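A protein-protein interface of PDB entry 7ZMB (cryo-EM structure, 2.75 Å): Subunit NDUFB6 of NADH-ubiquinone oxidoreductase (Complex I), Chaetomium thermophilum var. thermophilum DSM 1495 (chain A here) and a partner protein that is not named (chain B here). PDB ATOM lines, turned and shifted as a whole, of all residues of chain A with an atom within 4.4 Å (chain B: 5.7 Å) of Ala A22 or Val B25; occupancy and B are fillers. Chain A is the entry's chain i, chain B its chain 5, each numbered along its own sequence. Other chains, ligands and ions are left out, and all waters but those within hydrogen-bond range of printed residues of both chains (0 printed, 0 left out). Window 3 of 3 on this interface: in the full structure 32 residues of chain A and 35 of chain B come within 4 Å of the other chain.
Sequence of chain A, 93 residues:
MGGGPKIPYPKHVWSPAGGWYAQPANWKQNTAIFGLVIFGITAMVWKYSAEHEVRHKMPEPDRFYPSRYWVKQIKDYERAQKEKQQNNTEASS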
ATOM      1  N   GLY A  18     -11.197   0.543 -18.145  1.00  0.00           N
ATOM      2  CA  GLY A  18     -11.518   1.946 -18.013  1.00  0.00           C
ATOM      3  C   GLY A  18     -12.930   2.347 -18.360  1.00  0.00           C
ATOM      4  O   GLY A  18     -13.517   3.199 -17.685  1.00  0.00           O
ATOM      5  N   GLY A  19     -13.500   1.746 -19.390  1.00  0.00           N
ATOM      6  CA  GLY A  19     -14.836   2.137 -19.781  1.00  0.00           C
ATOM      7  C   GLY A  19     -14.836   2.792 -21.143  1.00  0.00           C
ATOM      8  O   GLY A  19     -14.061   2.394 -22.014  1.00  0.00           O
ATOM      9  N   TRP A  20     -15.682   3.801 -21.349  1.00  0.00           N
ATOM     10  CA  TRP A  20     -15.832   4.327 -22.699  1.00  0.00           C
ATOM     11  C   TRP A  20     -14.799   5.398 -23.022  1.00  0.00           C
ATOM     12  O   TRP A  20     -13.950   5.189 -23.884  1.00  0.00           O
ATOM     13  CB  TRP A  20     -17.250   4.853 -22.907  1.00  0.00           C
ATOM     14  CG  TRP A  20     -18.138   3.787 -23.380  1.00  0.00           C
ATOM     15  CD1 TRP A  20     -18.531   3.556 -24.656  1.00  0.00           C
ATOM     16  CD2 TRP A  20     -18.720   2.760 -22.583  1.00  0.00           C
ATOM     17  NE1 TRP A  20     -19.343   2.454 -24.706  1.00  0.00           N
ATOM     18  CE2 TRP A  20     -19.475   1.945 -23.443  1.00  0.00           C
ATOM     19  CE3 TRP A  20     -18.687   2.458 -21.220  1.00  0.00           C
ATOM     20  CZ2 TRP A  20     -20.191   0.857 -22.989  1.00  0.00           C
ATOM     21  CZ3 TRP A  20     -19.395   1.379 -20.772  1.00  0.00           C
ATOM     22  CH2 TRP A  20     -20.142   0.590 -21.650  1.00  0.00           C
ATOM     23  N   TYR A  21     -14.816   6.521 -22.319  1.00  0.00           N
ATOM     24  CA  TYR A  21     -13.819   7.537 -22.637  1.00  0.00           C
ATOM     25  C   TYR A  21     -12.998   7.845 -21.400  1.00  0.00           C
ATOM     26  O   TYR A  21     -12.782   9.011 -21.056  1.00  0.00           O
ATOM     27  CB  TYR A  21     -14.484   8.792 -23.194  1.00  0.00           C
ATOM     28  CG  TYR A  21     -15.227   8.543 -24.482  1.00  0.00           C
ATOM     29  CD1 TYR A  21     -16.542   8.115 -24.473  1.00  0.00           C
ATOM     30  CD2 TYR A  21     -14.613   8.736 -25.706  1.00  0.00           C
ATOM     31  CE1 TYR A  21     -17.219   7.881 -25.639  1.00  0.00           C
ATOM     32  CE2 TYR A  21     -15.282   8.507 -26.881  1.00  0.00           C
ATOM     33  CZ  TYR A  21     -16.585   8.082 -26.844  1.00  0.00           C
ATOM     34  OH  TYR A  21     -17.259   7.853 -28.019  1.00  0.00           O
ATOM     35  N   ALA A  22     -12.532   6.795 -20.738  1.00  0.00           N
ATOM     36  CA  ALA A  22     -12.015   6.914 -19.387  1.00  0.00           C
ATOM     37  C   ALA A  22     -10.700   7.679 -19.341  1.00  0.00           C
ATOM     38  O   ALA A  22      -9.762   7.378 -20.082  1.00  0.00           O
ATOM     39  CB  ALA A  22     -11.824   5.532 -18.784  1.00  0.00           C
ATOM     40  N   GLN A  23     -10.648   8.674 -18.468  1.00  0.00           N
ATOM     41  CA  GLN A  23      -9.389   9.228 -18.002  1.00  0.00           C
ATOM     42  C   GLN A  23      -9.614   9.892 -16.653  1.00  0.00           C
ATOM     43  O   GLN A  23     -10.426  10.818 -16.544  1.00  0.00           O
ATOM     44  CB  GLN A  23      -8.795  10.220 -19.001  1.00  0.00           C
ATOM     45  CG  GLN A  23      -7.385  10.636 -18.628  1.00  0.00           C
ATOM     46  CD  GLN A  23      -6.557  11.041 -19.824  1.00  0.00           C
ATOM     47  OE1 GLN A  23      -5.330  10.935 -19.814  1.00  0.00           O
ATOM     48  NE2 GLN A  23      -7.224  11.509 -20.866  1.00  0.00           N
ATOM     49  N   GLY B  20      -5.989   0.074 -16.982  1.00  0.00           N
ATOM     50  CA  GLY B  20      -6.277   1.194 -17.858  1.00  0.00           C
ATOM     51  C   GLY B  20      -7.287   2.153 -17.279  1.00  0.00           C
ATOM     52  O   GLY B  20      -7.311   3.324 -17.658  1.00  0.00           O
ATOM     53  N   ARG B  21      -8.129   1.673 -16.367  1.00  0.00           N
ATOM     54  CA  ARG B  21      -8.969   2.564 -15.584  1.00  0.00           C
ATOM     55  C   ARG B  21      -8.133   3.534 -14.760  1.00  0.00           C
ATOM     56  O   ARG B  21      -8.532   4.686 -14.568  1.00  0.00           O
ATOM     57  CB  ARG B  21      -9.878   1.736 -14.675  1.00  0.00           C
ATOM     58  CG  ARG B  21     -11.095   2.464 -14.196  1.00  0.00           C
ATOM     59  CD  ARG B  21     -11.915   1.610 -13.267  1.00  0.00           C
ATOM     60  NE  ARG B  21     -12.885   2.397 -12.516  1.00  0.00           N
ATOM     61  CZ  ARG B  21     -14.127   2.622 -12.916  1.00  0.00           C
ATOM     62  NH1 ARG B  21     -14.553   2.120 -14.062  1.00  0.00           N
ATOM     63  NH2 ARG B  21     -14.939   3.350 -12.170  1.00  0.00           N
ATOM     64  N   VAL B  23      -4.873   4.542 -15.310  1.00  0.00           N
ATOM     65  CA  VAL B  23      -3.803   5.284 -15.965  1.00  0.00           C
ATOM     66  C   VAL B  23      -4.404   6.155 -17.054  1.00  0.00           C
ATOM     67  O   VAL B  23      -3.737   7.048 -17.585  1.00  0.00           O
ATOM     68  CB  VAL B  23      -2.714   4.354 -16.534  1.00  0.00           C
ATOM     69  CG1 VAL B  23      -1.973   3.650 -15.412  1.00  0.00           C
ATOM     70  CG2 VAL B  23      -3.319   3.340 -17.490  1.00  0.00           C
ATOM     71  N   GLY B  24      -5.659   5.901 -17.398  1.00  0.00           N
ATOM     72  CA  GLY B  24      -6.331   6.740 -18.366  1.00  0.00           C
ATOM     73  C   GLY B  24      -5.851   6.527 -19.786  1.00  0.00           C
ATOM     74  O   GLY B  24      -4.887   5.798 -20.025  1.00  0.00           O
ATOM     75  N   VAL B  25      -6.522   7.174 -20.739  1.00  0.00           N
ATOM     76  CA  VAL B  25      -6.232   6.935 -22.147  1.00  0.00           C
ATOM     77  C   VAL B  25      -4.812   7.356 -22.475  1.00  0.00           C
ATOM     78  O   VAL B  25      -4.042   6.597 -23.076  1.00  0.00           O
ATOM     79  CB  VAL B  25      -7.252   7.668 -23.034  1.00  0.00           C
ATOM     80  CG1 VAL B  25      -6.726   7.797 -24.451  1.00  0.00           C
ATOM     81  CG2 VAL B  25      -8.572   6.935 -23.028  1.00  0.00           C
ATOM     82  N   SER B  26      -4.440   8.571 -22.084  1.00  0.00           N
ATOM     83  CA  SER B  26      -3.111   9.068 -22.412  1.00  0.00           C
ATOM     84  C   SER B  26      -2.028   8.333 -21.634  1.00  0.00           C
ATOM     85  O   SER B  26      -0.926   8.119 -22.149  1.00  0.00           O
ATOM     86  CB  SER B  26      -3.061  10.572 -22.169  1.00  0.00           C
ATOM     87  OG  SER B  26      -3.213  10.867 -20.800  1.00  0.00           O
ATOM     88  N   GLY B  27      -2.317   7.939 -20.395  1.00  0.00           N
ATOM     89  CA  GLY B  27      -1.354   7.155 -19.646  1.00  0.00           C
ATOM     90  C   GLY B  27      -1.148   5.777 -20.240  1.00  0.00           C
ATOM     91  O   GLY B  27      -0.019   5.281 -20.308  1.00  0.00           O
ATOM     92  N   ALA B  28      -2.235   5.141 -20.680  1.00  0.00           N
ATOM     93  CA  ALA B  28      -2.121   3.847 -21.334  1.00  0.00           C
ATOM     94  C   ALA B  28      -1.271   3.949 -22.590  1.00  0.00           C
ATOM     95  O   ALA B  28      -0.480   3.047 -22.889  1.00  0.00           O
ATOM     96  CB  ALA B  28      -3.505   3.303 -21.661  1.00  0.00           C
ATOM     97  N   GLN B  29      -1.411   5.044 -23.334  1.00  0.00           N
ATOM     98  CA  GLN B  29      -0.597   5.232 -24.528  1.00  0.00           C
ATOM     99  C   GLN B  29       0.862   5.472 -24.167  1.00  0.00           C
ATOM    100  O   GLN B  29       1.765   4.875 -24.763  1.00  0.00           O
ATOM    101  CB  GLN B  29      -1.145   6.392 -25.358  1.00  0.00           C
ATOM    102  CG  GLN B  29      -2.550   6.168 -25.859  1.00  0.00           C
ATOM    103  CD  GLN B  29      -3.208   7.440 -26.315  1.00  0.00           C
ATOM    104  OE1 GLN B  29      -3.689   8.227 -25.503  1.00  0.00           O
ATOM    105  NE2 GLN B  29      -3.244   7.650 -27.627  1.00  0.00           N
ATOM    106  N   LEU B  30       1.114   6.340 -23.192  1.00  0.00           N
ATOM    107  CA  LEU B  30       2.492   6.685 -22.857  1.00  0.00           C
ATOM    108  C   LEU B  30       3.242   5.484 -22.294  1.00  0.00           C
ATOM    109  O   LEU B  30       4.412   5.267 -22.626  1.00  0.00           O
ATOM    110  CB  LEU B  30       2.508   7.860 -21.878  1.00  0.00           C
ATOM    111  CG  LEU B  30       3.840   8.522 -21.515  1.00  0.00           C
ATOM    112  CD1 LEU B  30       3.595   9.964 -21.120  1.00  0.00           C
ATOM    113  CD2 LEU B  30       4.554   7.793 -20.386  1.00  0.00           C
ATOM    114  N   PRO B 108     -13.802   5.211 -28.461  1.00  0.00           N
ATOM    115  CA  PRO B 108     -13.889   5.268 -27.000  1.00  0.00           C
ATOM    116  C   PRO B 108     -12.882   4.365 -26.314  1.00  0.00           C
ATOM    117  O   PRO B 108     -12.011   4.826 -25.572  1.00  0.00           O
ATOM    118  CB  PRO B 108     -15.327   4.815 -26.713  1.00  0.00           C
ATOM    119  CG  PRO B 108     -15.796   4.161 -27.943  1.00  0.00           C
ATOM    120  CD  PRO B 108     -15.071   4.797 -29.074  1.00  0.00           C
ATOM    121  N   ASN B 110     -10.013   3.022 -26.072  1.00  0.00           N
ATOM    122  CA  ASN B 110      -8.718   3.288 -26.664  1.00  0.00           C
ATOM    123  C   ASN B 110      -7.588   2.677 -25.844  1.00  0.00           C
ATOM    124  O   ASN B 110      -6.465   2.563 -26.335  1.00  0.00           O
ATOM    125  CB  ASN B 110      -8.542   4.811 -26.790  1.00  0.00           C
ATOM    126  CG  ASN B 110      -7.335   5.218 -27.611  1.00  0.00           C
ATOM    127  OD1 ASN B 110      -6.580   4.389 -28.097  1.00  0.00           O
ATOM    128  ND2 ASN B 110      -7.158   6.523 -27.776  1.00  0.00           N
ATOM    129  N   GLN B 111      -7.869   2.264 -24.613  1.00  0.00           N
ATOM    130  CA  GLN B 111      -6.830   1.703 -23.761  1.00  0.00           C
ATOM    131  C   GLN B 111      -6.952   0.190 -23.622  1.00  0.00           C
ATOM    132  O   GLN B 111      -6.003  -0.468 -23.183  1.00  0.00           O
ATOM    133  CB  GLN B 111      -6.865   2.400 -22.412  1.00  0.00           C
ATOM    134  CG  GLN B 111      -8.218   2.445 -21.795  1.00  0.00           C
ATOM    135  CD  GLN B 111      -8.301   3.487 -20.717  1.00  0.00           C
ATOM    136  OE1 GLN B 111      -7.293   4.058 -20.326  1.00  0.00           O
ATOM    137  NE2 GLN B 111      -9.502   3.736 -20.220  1.00  0.00           N
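Of the 6 printed residues of chain A, 5 touch a printed residue of chain B. Printed residues of chain A that touch a printed residue of chain B: Gly A18, Trp A20, Tyr A21, Ala A22 and Gln A23. Hydrophobic or aromatic side chains of chain A within 4 Å of the printed part of chain B: Tyr A21 and Ala A22. Of the 13 printed residues of chain B, 6 touch a printed residue of chain A. Among the printed residues, no Asp or Glu carboxylate lies within 4 Å of a Lys or Arg side-chain nitrogen of the other chain.
N of Val B25 sits close to O of Ala A22, at 3.3 Å. The side-chain amide oxygen (OE1) of Gln A23 sits close to the backbone NH (N) of Ser B26, at 3.4 Å. O of Pro B108 lies close to O of Trp A20.
Among the printed residues, pairs that only touch across the chains: Gly A18 with Arg B21, Gly A18 with Gln B111, Tyr A21 with Pro B108, Ala A22 with Gly B24, Ala A22 with Gln B111, Gln A23 with Gly B24 and Gln A23 with Val B25.
The backbone NH of Val B25 is in hydrogen-bond range of the side-chain amide oxygen of Gln B111 (3.2 Å). OE1 of Gln B111 lies close to O of Gly B20 (2.8 Å). The side-chain amide oxygen (OE1) of Gln B111 lies close to the backbone carbonyl oxygen (O) of Gly B24 (3.0 Å). The side-chain amide oxygen (OE1) of Gln B29 sits close to the backbone carbonyl oxygen (O) of Val B25, at 2.9 Å.
Of the printed residues of chain B, Tyr A21 touches Pro B108 (3.5 Å). Of chain B, only Gly B24, Val B25 and Gln B111 come within 4 Å of Ala A22. Of the printed residues of chain A, Val B25 touches Ala A22 (3.2 Å) and Gln A23 (3.97 Å). Gln B29 touches none of the printed residues of chain A. Printed residues of chain A within 4 Å of Gln B111: Gly A18 (3.5 Å) and Ala A22 (3.3 Å). The nearest residue of chain B that does not touch Ala A22 is Gly B20 (5.1 Å). The nearest printed residue of chain A that does not touch Val B25 is Tyr A21 (4.8 Å). The nearest printed residue of chain A that does not touch Pro B108 is Gly A19 (4.8 Å).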
